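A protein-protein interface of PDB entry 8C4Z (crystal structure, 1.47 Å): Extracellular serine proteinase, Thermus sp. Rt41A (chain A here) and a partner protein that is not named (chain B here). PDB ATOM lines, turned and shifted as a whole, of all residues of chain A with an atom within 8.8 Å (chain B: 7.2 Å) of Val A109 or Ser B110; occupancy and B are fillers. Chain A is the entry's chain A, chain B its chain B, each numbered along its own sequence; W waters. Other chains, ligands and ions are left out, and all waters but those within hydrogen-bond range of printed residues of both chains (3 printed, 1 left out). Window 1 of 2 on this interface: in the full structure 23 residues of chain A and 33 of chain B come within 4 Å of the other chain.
The backbone NH (N) of Ile A21 is in hydrogen-bond range of the backbone carbonyl oxygen (O) of Asp A106 (2.9 Å).
The side-chain carboxylate (OE2) of Glu A85 lies within salt-bridge range of the guanidinium group (NH1) of Arg A24 (2.9 Å).
The guanidinium group (NE) of Arg A24 lies within salt-bridge range of the side-chain carboxylate (OD2) of Asp A106 (2.8 Å).
The backbone NH (N) of Asp A72 is in hydrogen-bond range of the backbone carbonyl oxygen (O) of Ala A83 (2.9 Å).
O of Ala A105 is in hydrogen-bond range of NE2 of Gln A107 (3.1 Å).
The backbone carbonyl oxygen (O) of Ser B110 sits at hydrogen-bond distance from the side-chain hydroxyl (OG) of Ser B113 (2.9 Å).
Water W1 bridges the side-chain amide nitrogen of Asn B111 (2.7 Å) and the backbone carbonyl oxygen of Ala A105 (2.7 Å).
Water W3 lies within hydrogen-bond range of the backbone carbonyl oxygen (O) of Glu A108 (2.8 Å) and the backbone NH (N) of Gly B138 (2.9 Å).
Water W2 lies within hydrogen-bond range of the side-chain amino group (NZ) of Lys A73 (3.1 Å) and the backbone carbonyl oxygen (O) of Ile B64 (3.5 Å).
Of the printed residues of chain B, Val A109 touches Ser B108 (3.6 Å), Gly B109 (2.9 Å), Ser B110 (3.98 Å), Asn B111 (3.3 Å), Leu B135 (3.9 Å) and Gly B136 (3.5 Å).
Ser B110 touches just these residues of chain A: Ile A21 (3.7 Å), Asp A106 (3.4 Å), Gln A107 (3.2 Å) and Val A109 (3.98 Å).
Gly B136 touches just these residues of chain A: Val A109, Arg A110 and Phe A112.
Of the printed residues of chain B, Gln A107 touches Ser B110 (3.2 Å) and Asn B111 (2.9 Å).
Printed residues of chain B within 4 Å of Ile A26: Asn B111 (3.9 Å), Ser B112 (3.8 Å) and Ile B115 (3.99 Å).
Printed residues of chain B within 4 Å of Arg A110: Gly B107, Leu B135 and Gly B136.
Of the printed residues of chain A, Leu B103 touches Ala A111 (3.8 Å).
Printed residues of chain B within 4 Å of Lys A73: Ala B116 (3.7 Å).
Asp B104 touches none of the printed residues of chain A.
Asp A72 touches none of the printed residues of chain B.
NH2 of Arg A24 sits at hydrogen-bond distance from OG of Ser B112 (3.2 Å).
The backbone carbonyl oxygen (O) of Ser B112 sits at hydrogen-bond distance from the side-chain hydroxyl (OH) of Tyr A75 (2.8 Å).
OD1 of Asp A106 sits at hydrogen-bond distance from N of Asn B111 (3.3 Å).
The side-chain hydroxyl (OG) of Ser B112 sits at hydrogen-bond distance from the side-chain carboxylate (OD2) of Asp A106 (2.7 Å).
The backbone carbonyl oxygen of Gln A107 sits at hydrogen-bond distance from the backbone NH of Asn B111 (2.9 Å).
The side-chain hydroxyl (OG) of Ser B108 lies within hydrogen-bond range of the side-chain carboxylate (OE1) of Glu A108 (2.8 Å).
N of Val A109 lies within hydrogen-bond range of O of Gly B109 (2.9 Å).
The backbone carbonyl oxygen of Arg A110 sits at hydrogen-bond distance from the backbone NH of Gly B136 (3.2 Å).
The backbone carbonyl oxygen (O) of Gly B107 is in hydrogen-bond range of the backbone NH (N) of Ala A111 (3.1 Å).
Ile A21 touches Ser B110 (CD1 to CB, 3.7 Å).
CD1 of Ile A26 touches CD1 of Ile B115, at 3.99 Å.
CB of Ala B116 touches CD of Lys A73 (3.7 Å).
Tyr A75 touches Ala B116.
CB of Ser B112 touches CB of Ala A83, 3.7 Å away.
Gly B109 touches Glu A108.
CA of Ser B108 touches O of Val A109, at 3.6 Å.
CD1 of Leu B135 touches CG1 of Val A109, at 3.9 Å.
Phe A112 touches Gly B136.
Gly B137 touches Phe A112.
Hydrophobic or aromatic side chains of chain B that line the printed part of chain A: Leu B103, Ile B115, Ala B116 and Leu B135.
Of the 18 printed residues of chain A, 13 touch a printed residue of chain B.
Printed residues of chain A that touch a printed residue of chain B: Ile A21, Arg A24, Ile A26, Lys A73, Tyr A75, Ala A83, Asp A106, Gln A107, Glu A108, Val A109, Arg A110, Ala A111 and Phe A112.
Hydrophobic or aromatic side chains of chain A within 4 Å of the printed part of chain B: Ile A21, Ile A26, Tyr A75, Ala A83, Val A109, Ala A111 and Phe A112.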
ATOM      1  N   GLU A  19      -4.182  -0.354  10.313  1.00  0.00           N
ATOM      2  CA  GLU A  19      -3.777   0.963  10.781  1.00  0.00           C
ATOM      3  C   GLU A  19      -2.302   1.031  11.175  1.00  0.00           C
ATOM      4  O   GLU A  19      -1.869   2.058  11.705  1.00  0.00           O
ATOM      5  CB  GLU A  19      -4.673   1.399  11.944  1.00  0.00           C
ATOM      6  CG  GLU A  19      -6.143   1.523  11.565  1.00  0.00           C
ATOM      7  CD  GLU A  19      -6.902   0.211  11.737  1.00  0.00           C
ATOM      8  OE1 GLU A  19      -6.295  -0.768  12.237  1.00  0.00           O
ATOM      9  OE2 GLU A  19      -8.103   0.157  11.379  1.00  0.00           O
ATOM     10  N   ALA A  20      -1.524  -0.026  10.929  1.00  0.00           N
ATOM     11  CA  ALA A  20      -0.097   0.020  11.231  1.00  0.00           C
ATOM     12  C   ALA A  20       0.579   1.129  10.432  1.00  0.00           C
ATOM     13  O   ALA A  20       0.280   1.334   9.252  1.00  0.00           O
ATOM     14  CB  ALA A  20       0.564  -1.317  10.890  1.00  0.00           C
ATOM     15  N   ILE A  21       1.492   1.842  11.083  1.00  0.00           N
ATOM     16  CA  ILE A  21       2.239   2.935  10.469  1.00  0.00           C
ATOM     17  C   ILE A  21       3.591   2.380  10.034  1.00  0.00           C
ATOM     18  O   ILE A  21       4.376   1.963  10.897  1.00  0.00           O
ATOM     19  CB  ILE A  21       2.429   4.096  11.454  1.00  0.00           C
ATOM     20  CG1 ILE A  21       1.072   4.664  11.903  1.00  0.00           C
ATOM     21  CG2 ILE A  21       3.308   5.185  10.824  1.00  0.00           C
ATOM     22  CD1 ILE A  21       1.171   5.540  13.156  1.00  0.00           C
ATOM     23  N   ARG A  24       7.507   2.452  11.941  1.00  0.00           N
ATOM     24  CA  ARG A  24       7.456   3.067  13.257  1.00  0.00           C
ATOM     25  C   ARG A  24       7.036   2.026  14.288  1.00  0.00           C
ATOM     26  O   ARG A  24       6.130   1.220  14.038  1.00  0.00           O
ATOM     27  CB  ARG A  24       6.459   4.216  13.228  1.00  0.00           C
ATOM     28  CG  ARG A  24       6.540   5.117  14.408  1.00  0.00           C
ATOM     29  CD  ARG A  24       5.661   6.339  14.195  1.00  0.00           C
ATOM     30  NE  ARG A  24       5.618   7.131  15.412  1.00  0.00           N
ATOM     31  CZ  ARG A  24       6.482   8.095  15.690  1.00  0.00           C
ATOM     32  NH1 ARG A  24       7.410   8.460  14.816  1.00  0.00           N
ATOM     33  NH2 ARG A  24       6.409   8.710  16.866  1.00  0.00           N
ATOM     34  N   ILE A  26       6.900   0.827  18.742  1.00  0.00           N
ATOM     35  CA  ILE A  26       6.988   1.067  20.180  1.00  0.00           C
ATOM     36  C   ILE A  26       7.734  -0.113  20.801  1.00  0.00           C
ATOM     37  O   ILE A  26       7.264  -1.254  20.733  1.00  0.00           O
ATOM     38  CB  ILE A  26       5.593   1.248  20.808  1.00  0.00           C
ATOM     39  CG1 ILE A  26       4.870   2.434  20.157  1.00  0.00           C
ATOM     40  CG2 ILE A  26       5.685   1.423  22.333  1.00  0.00           C
ATOM     41  CD1 ILE A  26       3.378   2.518  20.467  1.00  0.00           C
ATOM     42  N   ASP A  72      11.677   9.199  18.921  1.00  0.00           N
ATOM     43  CA  ASP A  72      10.683  10.268  18.861  1.00  0.00           C
ATOM     44  C   ASP A  72      10.002  10.520  20.198  1.00  0.00           C
ATOM     45  O   ASP A  72       9.680  11.670  20.526  1.00  0.00           O
ATOM     46  CB  ASP A  72       9.601   9.905  17.830  1.00  0.00           C
ATOM     47  N   LYS A  73       9.747   9.463  20.965  1.00  0.00           N
ATOM     48  CA  LYS A  73       9.112   9.551  22.272  1.00  0.00           C
ATOM     49  C   LYS A  73       9.820   8.604  23.223  1.00  0.00           C
ATOM     50  O   LYS A  73      10.337   7.556  22.813  1.00  0.00           O
ATOM     51  CB  LYS A  73       7.625   9.175  22.213  1.00  0.00           C
ATOM     52  CG  LYS A  73       6.789  10.107  21.326  1.00  0.00           C
ATOM     53  CD  LYS A  73       6.740  11.520  21.945  1.00  0.00           C
ATOM     54  CE  LYS A  73       5.678  12.413  21.334  1.00  0.00           C
ATOM     55  NZ  LYS A  73       5.808  12.495  19.864  1.00  0.00           N
ATOM     56  N   TYR A  75       9.265   6.861  27.192  1.00  0.00           N
ATOM     57  CA  TYR A  75       8.268   6.606  28.220  1.00  0.00           C
ATOM     58  C   TYR A  75       8.946   6.093  29.475  1.00  0.00           C
ATOM     59  O   TYR A  75       9.778   5.176  29.404  1.00  0.00           O
ATOM     60  CB  TYR A  75       7.263   5.561  27.740  1.00  0.00           C
ATOM     61  CG  TYR A  75       6.725   5.827  26.350  1.00  0.00           C
ATOM     62  CD1 TYR A  75       6.080   7.028  26.046  1.00  0.00           C
ATOM     63  CD2 TYR A  75       6.848   4.863  25.336  1.00  0.00           C
ATOM     64  CE1 TYR A  75       5.576   7.269  24.771  1.00  0.00           C
ATOM     65  CE2 TYR A  75       6.342   5.093  24.068  1.00  0.00           C
ATOM     66  CZ  TYR A  75       5.706   6.292  23.788  1.00  0.00           C
ATOM     67  OH  TYR A  75       5.217   6.509  22.519  1.00  0.00           O
ATOM     68  N   ALA A  83       9.473   5.171  21.395  1.00  0.00           N
ATOM     69  CA  ALA A  83       8.928   5.130  20.045  1.00  0.00           C
ATOM     70  C   ALA A  83      10.050   5.488  19.080  1.00  0.00           C
ATOM     71  O   ALA A  83      10.724   6.514  19.257  1.00  0.00           O
ATOM     72  CB  ALA A  83       7.759   6.105  19.874  1.00  0.00           C
ATOM     73  N   GLU A  85      11.757   5.100  14.820  1.00  0.00           N
ATOM     74  CA  GLU A  85      11.597   4.838  13.392  1.00  0.00           C
ATOM     75  C   GLU A  85      12.916   4.242  12.917  1.00  0.00           C
ATOM     76  O   GLU A  85      13.941   4.933  12.901  1.00  0.00           O
ATOM     77  CB  GLU A  85      11.255   6.125  12.640  1.00  0.00           C
ATOM     78  CG  GLU A  85       9.847   6.621  12.939  1.00  0.00           C
ATOM     79  CD  GLU A  85       9.239   7.471  11.831  1.00  0.00           C
ATOM     80  OE1 GLU A  85       9.894   7.667  10.782  1.00  0.00           O
ATOM     81  OE2 GLU A  85       8.112   7.977  12.032  1.00  0.00           O
ATOM     82  N   ALA A 105       4.288  -2.562  16.306  1.00  0.00           N
ATOM     83  CA  ALA A 105       4.143  -1.554  15.268  1.00  0.00           C
ATOM     84  C   ALA A 105       3.248  -0.441  15.794  1.00  0.00           C
ATOM     85  O   ALA A 105       2.210  -0.704  16.407  1.00  0.00           O
ATOM     86  CB  ALA A 105       3.520  -2.180  14.020  1.00  0.00           C
ATOM     87  N   ASP A 106       3.669   0.804  15.587  1.00  0.00           N
ATOM     88  CA  ASP A 106       2.795   1.927  15.890  1.00  0.00           C
ATOM     89  C   ASP A 106       1.559   1.863  14.995  1.00  0.00           C
ATOM     90  O   ASP A 106       1.592   1.319  13.885  1.00  0.00           O
ATOM     91  CB  ASP A 106       3.545   3.240  15.674  1.00  0.00           C
ATOM     92  CG  ASP A 106       2.994   4.385  16.510  1.00  0.00           C
ATOM     93  OD1 ASP A 106       2.021   4.191  17.284  1.00  0.00           O
ATOM     94  OD2 ASP A 106       3.555   5.498  16.395  1.00  0.00           O
ATOM     95  N   GLN A 107       0.451   2.408  15.497  1.00  0.00           N
ATOM     96  CA  GLN A 107      -0.852   2.289  14.860  1.00  0.00           C
ATOM     97  C   GLN A 107      -1.557   3.629  14.906  1.00  0.00           C
ATOM     98  O   GLN A 107      -1.414   4.379  15.871  1.00  0.00           O
ATOM     99  CB  GLN A 107      -1.738   1.324  15.652  1.00  0.00           C
ATOM    100  CG  GLN A 107      -1.082  -0.011  15.958  1.00  0.00           C
ATOM    101  CD  GLN A 107      -1.148  -0.980  14.807  1.00  0.00           C
ATOM    102  OE1 GLN A 107      -2.108  -0.988  14.037  1.00  0.00           O
ATOM    103  NE2 GLN A 107      -0.114  -1.803  14.674  1.00  0.00           N
ATOM    104  N   GLU A 108      -2.358   3.905  13.880  1.00  0.00           N
ATOM    105  CA  GLU A 108      -3.157   5.124  13.866  1.00  0.00           C
ATOM    106  C   GLU A 108      -4.305   5.029  14.861  1.00  0.00           C
ATOM    107  O   GLU A 108      -4.915   3.970  15.027  1.00  0.00           O
ATOM    108  CB  GLU A 108      -3.714   5.380  12.468  1.00  0.00           C
ATOM    109  CG  GLU A 108      -3.812   6.860  12.121  1.00  0.00           C
ATOM    110  CD  GLU A 108      -4.714   7.112  10.936  1.00  0.00           C
ATOM    111  OE1 GLU A 108      -5.766   7.772  11.105  1.00  0.00           O
ATOM    112  OE2 GLU A 108      -4.377   6.629   9.835  1.00  0.00           O
ATOM    113  N   VAL A 109      -4.575   6.147  15.538  1.00  0.00           N
ATOM    114  CA  VAL A 109      -5.694   6.325  16.458  1.00  0.00           C
ATOM    115  C   VAL A 109      -6.516   7.502  15.951  1.00  0.00           C
ATOM    116  O   VAL A 109      -5.980   8.403  15.298  1.00  0.00           O
ATOM    117  CB  VAL A 109      -5.129   6.600  17.873  1.00  0.00           C
ATOM    118  CG1 VAL A 109      -6.168   7.207  18.799  1.00  0.00           C
ATOM    119  CG2 VAL A 109      -4.569   5.315  18.460  1.00  0.00           C
ATOM    120  N   ARG A 110      -7.824   7.489  16.230  1.00  0.00           N
ATOM    121  CA  ARG A 110      -8.706   8.573  15.808  1.00  0.00           C
ATOM    122  C   ARG A 110      -9.562   9.063  16.967  1.00  0.00           C
ATOM    123  O   ARG A 110      -9.862   8.316  17.901  1.00  0.00           O
ATOM    124  CB  ARG A 110      -9.650   8.141  14.663  1.00  0.00           C
ATOM    125  CG  ARG A 110      -8.928   7.712  13.398  1.00  0.00           C
ATOM    126  N   ALA A 111      -9.950  10.339  16.892  1.00  0.00           N
ATOM    127  CA  ALA A 111     -10.980  10.874  17.775  1.00  0.00           C
ATOM    128  C   ALA A 111     -12.303  10.148  17.544  1.00  0.00           C
ATOM    129  O   ALA A 111     -12.655   9.815  16.407  1.00  0.00           O
ATOM    130  CB  ALA A 111     -11.168  12.360  17.472  1.00  0.00           C
ATOM    131  N   PHE A 112     -13.044   9.922  18.629  1.00  0.00           N
ATOM    132  CA  PHE A 112     -14.332   9.202  18.588  1.00  0.00           C
ATOM    133  C   PHE A 112     -15.543  10.148  18.589  1.00  0.00           C
ATOM    134  O   PHE A 112     -16.667   9.801  19.025  1.00  0.00           O
ATOM    135  CB  PHE A 112     -14.434   8.212  19.762  1.00  0.00           C
ATOM    136  CG  PHE A 112     -13.675   6.922  19.553  1.00  0.00           C
ATOM    137  CD1 PHE A 112     -12.986   6.684  18.373  1.00  0.00           C
ATOM    138  CD2 PHE A 112     -13.655   5.953  20.538  1.00  0.00           C
ATOM    139  CE1 PHE A 112     -12.295   5.500  18.177  1.00  0.00           C
ATOM    140  CE2 PHE A 112     -12.969   4.767  20.358  1.00  0.00           C
ATOM    141  CZ  PHE A 112     -12.295   4.532  19.171  1.00  0.00           C
ATOM    142  OXT PHE A 112     -15.422  11.318  18.185  1.00  0.00           O
ATOM    143  N   ILE B  64       2.338  16.407  19.584  1.00  0.00           N
ATOM    144  CA  ILE B  64       2.440  16.618  18.146  1.00  0.00           C
ATOM    145  C   ILE B  64       3.641  17.494  17.806  1.00  0.00           C
ATOM    146  O   ILE B  64       4.318  17.274  16.799  1.00  0.00           O
ATOM    147  CB  ILE B  64       1.114  17.213  17.629  1.00  0.00           C
ATOM    148  CG1 ILE B  64      -0.062  16.284  17.940  1.00  0.00           C
ATOM    149  CG2 ILE B  64       1.193  17.503  16.138  1.00  0.00           C
ATOM    150  CD1 ILE B  64       0.075  14.896  17.359  1.00  0.00           C
ATOM    151  N   VAL B 102      -2.698  14.948  21.666  1.00  0.00           N
ATOM    152  CA  VAL B 102      -2.141  13.724  21.095  1.00  0.00           C
ATOM    153  C   VAL B 102      -2.648  13.448  19.691  1.00  0.00           C
ATOM    154  O   VAL B 102      -2.173  12.495  19.048  1.00  0.00           O
ATOM    155  CB  VAL B 102      -2.374  12.497  22.011  1.00  0.00           C
ATOM    156  CG1 VAL B 102      -1.844  12.766  23.424  1.00  0.00           C
ATOM    157  CG2 VAL B 102      -3.853  12.115  22.034  1.00  0.00           C
ATOM    158  N   LEU B 103      -3.617  14.222  19.204  1.00  0.00           N
ATOM    159  CA  LEU B 103      -4.158  14.097  17.859  1.00  0.00           C
ATOM    160  C   LEU B 103      -3.914  15.413  17.141  1.00  0.00           C
ATOM    161  O   LEU B 103      -3.919  16.484  17.762  1.00  0.00           O
ATOM    162  CB  LEU B 103      -5.673  13.836  17.897  1.00  0.00           C
ATOM    163  CG  LEU B 103      -6.120  12.653  18.762  1.00  0.00           C
ATOM    164  CD1 LEU B 103      -7.633  12.601  18.808  1.00  0.00           C
ATOM    165  CD2 LEU B 103      -5.565  11.353  18.197  1.00  0.00           C
ATOM    166  N   ASP B 104      -3.703  15.316  15.831  1.00  0.00           N
ATOM    167  CA  ASP B 104      -3.379  16.467  14.992  1.00  0.00           C
ATOM    168  C   ASP B 104      -4.634  17.269  14.625  1.00  0.00           C
ATOM    169  O   ASP B 104      -5.736  17.040  15.138  1.00  0.00           O
ATOM    170  CB  ASP B 104      -2.544  16.012  13.797  1.00  0.00           C
ATOM    171  CG  ASP B 104      -3.338  15.183  12.788  1.00  0.00           C
ATOM    172  OD1 ASP B 104      -4.585  15.162  12.831  1.00  0.00           O
ATOM    173  OD2 ASP B 104      -2.692  14.541  11.926  1.00  0.00           O
ATOM    174  N   GLY B 107      -7.704  15.290  13.679  1.00  0.00           N
ATOM    175  CA  GLY B 107      -8.210  14.318  14.627  1.00  0.00           C
ATOM    176  C   GLY B 107      -7.510  12.983  14.603  1.00  0.00           C
ATOM    177  O   GLY B 107      -8.030  12.012  15.168  1.00  0.00           O
ATOM    178  N   SER B 108      -6.338  12.900  13.983  1.00  0.00           N
ATOM    179  CA  SER B 108      -5.603  11.651  13.852  1.00  0.00           C
ATOM    180  C   SER B 108      -4.306  11.711  14.647  1.00  0.00           C
ATOM    181  O   SER B 108      -3.678  12.768  14.774  1.00  0.00           O
ATOM    182  CB  SER B 108      -5.280  11.355  12.384  1.00  0.00           C
ATOM    183  OG  SER B 108      -4.680  10.078  12.236  1.00  0.00           O
ATOM    184  N   GLY B 109      -3.918  10.568  15.175  1.00  0.00           N
ATOM    185  CA  GLY B 109      -2.675  10.446  15.891  1.00  0.00           C
ATOM    186  C   GLY B 109      -2.203   9.015  15.861  1.00  0.00           C
ATOM    187  O   GLY B 109      -2.580   8.229  14.991  1.00  0.00           O
ATOM    188  N   SER B 110      -1.381   8.660  16.838  1.00  0.00           N
ATOM    189  CA  SER B 110      -0.828   7.318  16.891  1.00  0.00           C
ATOM    190  C   SER B 110      -0.880   6.793  18.317  1.00  0.00           C
ATOM    191  O   SER B 110      -1.001   7.553  19.278  1.00  0.00           O
ATOM    192  CB  SER B 110       0.625   7.312  16.410  1.00  0.00           C
ATOM    193  OG  SER B 110       1.409   8.169  17.224  1.00  0.00           O
ATOM    194  N   ASN B 111      -0.763   5.471  18.445  1.00  0.00           N
ATOM    195  CA  ASN B 111      -0.541   4.888  19.761  1.00  0.00           C
ATOM    196  C   ASN B 111       0.626   5.570  20.461  1.00  0.00           C
ATOM    197  O   ASN B 111       0.546   5.873  21.653  1.00  0.00           O
ATOM    198  CB  ASN B 111      -0.286   3.379  19.655  1.00  0.00           C
ATOM    199  CG  ASN B 111      -1.564   2.573  19.495  1.00  0.00           C
ATOM    200  OD1 ASN B 111      -2.656   3.051  19.795  1.00  0.00           O
ATOM    201  ND2 ASN B 111      -1.428   1.333  19.034  1.00  0.00           N
ATOM    202  N   SER B 112       1.715   5.841  19.733  1.00  0.00           N
ATOM    203  CA  SER B 112       2.885   6.439  20.375  1.00  0.00           C
ATOM    204  C   SER B 112       2.592   7.839  20.932  1.00  0.00           C
ATOM    205  O   SER B 112       3.092   8.196  22.006  1.00  0.00           O
ATOM    206  CB  SER B 112       4.104   6.414  19.445  1.00  0.00           C
ATOM    207  OG  SER B 112       3.957   7.304  18.351  1.00  0.00           O
ATOM    208  N   SER B 113       1.772   8.642  20.240  1.00  0.00           N
ATOM    209  CA  SER B 113       1.439   9.964  20.774  1.00  0.00           C
ATOM    210  C   SER B 113       0.500   9.857  21.970  1.00  0.00           C
ATOM    211  O   SER B 113       0.648  10.598  22.955  1.00  0.00           O
ATOM    212  CB  SER B 113       0.835  10.864  19.690  1.00  0.00           C
ATOM    213  OG  SER B 113      -0.455  10.420  19.293  1.00  0.00           O
ATOM    214  N   VAL B 114      -0.477   8.949  21.904  1.00  0.00           N
ATOM    215  CA  VAL B 114      -1.396   8.779  23.026  1.00  0.00           C
ATOM    216  C   VAL B 114      -0.638   8.321  24.263  1.00  0.00           C
ATOM    217  O   VAL B 114      -0.857   8.826  25.370  1.00  0.00           O
ATOM    218  CB  VAL B 114      -2.537   7.812  22.667  1.00  0.00           C
ATOM    219  CG1 VAL B 114      -3.464   7.622  23.875  1.00  0.00           C
ATOM    220  CG2 VAL B 114      -3.322   8.326  21.441  1.00  0.00           C
ATOM    221  N   ILE B 115       0.259   7.349  24.095  1.00  0.00           N
ATOM    222  CA  ILE B 115       1.044   6.856  25.225  1.00  0.00           C
ATOM    223  C   ILE B 115       1.936   7.961  25.792  1.00  0.00           C
ATOM    224  O   ILE B 115       2.118   8.064  27.014  1.00  0.00           O
ATOM    225  CB  ILE B 115       1.821   5.586  24.828  1.00  0.00           C
ATOM    226  CG1 ILE B 115       0.835   4.461  24.470  1.00  0.00           C
ATOM    227  CG2 ILE B 115       2.792   5.171  25.931  1.00  0.00           C
ATOM    228  CD1 ILE B 115       1.519   3.219  23.926  1.00  0.00           C
ATOM    229  N   ALA B 116       2.491   8.814  24.920  1.00  0.00           N
ATOM    230  CA  ALA B 116       3.257   9.970  25.393  1.00  0.00           C
ATOM    231  C   ALA B 116       2.403  10.887  26.267  1.00  0.00           C
ATOM    232  O   ALA B 116       2.859  11.367  27.310  1.00  0.00           O
ATOM    233  CB  ALA B 116       3.860  10.745  24.215  1.00  0.00           C
ATOM    234  N   LEU B 135     -11.199   8.818  22.420  1.00  0.00           N
ATOM    235  CA  LEU B 135     -10.443   8.379  21.253  1.00  0.00           C
ATOM    236  C   LEU B 135     -10.108   6.912  21.454  1.00  0.00           C
ATOM    237  O   LEU B 135     -10.269   6.371  22.548  1.00  0.00           O
ATOM    238  CB  LEU B 135      -9.174   9.226  21.060  1.00  0.00           C
ATOM    239  CG  LEU B 135      -8.138   9.330  22.195  1.00  0.00           C
ATOM    240  CD1 LEU B 135      -7.354   8.039  22.420  1.00  0.00           C
ATOM    241  CD2 LEU B 135      -7.172  10.481  21.952  1.00  0.00           C
ATOM    242  N   GLY B 136      -9.598   6.281  20.402  1.00  0.00           N
ATOM    243  CA  GLY B 136      -9.202   4.893  20.519  1.00  0.00           C
ATOM    244  C   GLY B 136      -8.835   4.294  19.174  1.00  0.00           C
ATOM    245  O   GLY B 136      -8.736   4.989  18.156  1.00  0.00           O
ATOM    246  N   GLY B 137      -8.621   2.986  19.201  1.00  0.00           N
ATOM    247  CA  GLY B 137      -8.232   2.280  18.004  1.00  0.00           C
ATOM    248  C   GLY B 137      -8.223   0.787  18.228  1.00  0.00           C
ATOM    249  O   GLY B 137      -8.891   0.267  19.128  1.00  0.00           O
ATOM    250  N   GLY B 138      -7.449   0.100  17.395  1.00  0.00           N
ATOM    251  CA  GLY B 138      -7.341  -1.337  17.512  1.00  0.00           C
ATOM    252  C   GLY B 138      -6.670  -1.764  18.804  1.00  0.00           C
ATOM    253  O   GLY B 138      -6.007  -0.982  19.493  1.00  0.00           O
ATOM    254  N   LEU B 143      -0.818   0.254  24.709  1.00  0.00           N
ATOM    255  CA  LEU B 143      -1.747   1.300  25.114  1.00  0.00           C
ATOM    256  C   LEU B 143      -2.535   0.881  26.350  1.00  0.00           C
ATOM    257  O   LEU B 143      -2.744   1.686  27.272  1.00  0.00           O
ATOM    258  CB  LEU B 143      -2.675   1.655  23.956  1.00  0.00           C
ATOM    259  CG  LEU B 143      -3.741   2.717  24.258  1.00  0.00           C
ATOM    260  CD1 LEU B 143      -3.102   3.989  24.803  1.00  0.00           C
ATOM    261  CD2 LEU B 143      -4.580   3.022  23.012  1.00  0.00           C
ATOM    262  N   SER B 172      -8.914  -0.877  21.940  1.00  0.00           N
ATOM    263  CA  SER B 172      -8.176  -0.245  23.026  1.00  0.00           C
ATOM    264  C   SER B 172      -8.379   1.261  22.988  1.00  0.00           C
ATOM    265  O   SER B 172      -8.388   1.864  21.908  1.00  0.00           O
ATOM    266  CB  SER B 172      -6.670  -0.533  22.923  1.00  0.00           C
ATOM    267  OG  SER B 172      -6.394  -1.878  23.286  1.00  0.00           O
ATOM    268  N   PRO B 173      -8.505   1.909  24.145  1.00  0.00           N
ATOM    269  CA  PRO B 173      -8.453   1.348  25.495  1.00  0.00           C
ATOM    270  C   PRO B 173      -9.819   0.918  26.041  1.00  0.00           C
ATOM    271  O   PRO B 173      -9.914   0.661  27.236  1.00  0.00           O
ATOM    272  CB  PRO B 173      -7.901   2.514  26.321  1.00  0.00           C
ATOM    273  CG  PRO B 173      -8.436   3.734  25.605  1.00  0.00           C
ATOM    274  CD  PRO B 173      -8.449   3.383  24.142  1.00  0.00           C
HETATM  275  O   HOH W   1       1.070   0.293  18.687  1.00  0.00           O
HETATM  276  O   HOH W   2       6.459  15.245  18.680  1.00  0.00           O
HETATM  277  O   HOH W   3      -5.275   1.456  16.086  1.00  0.00           O
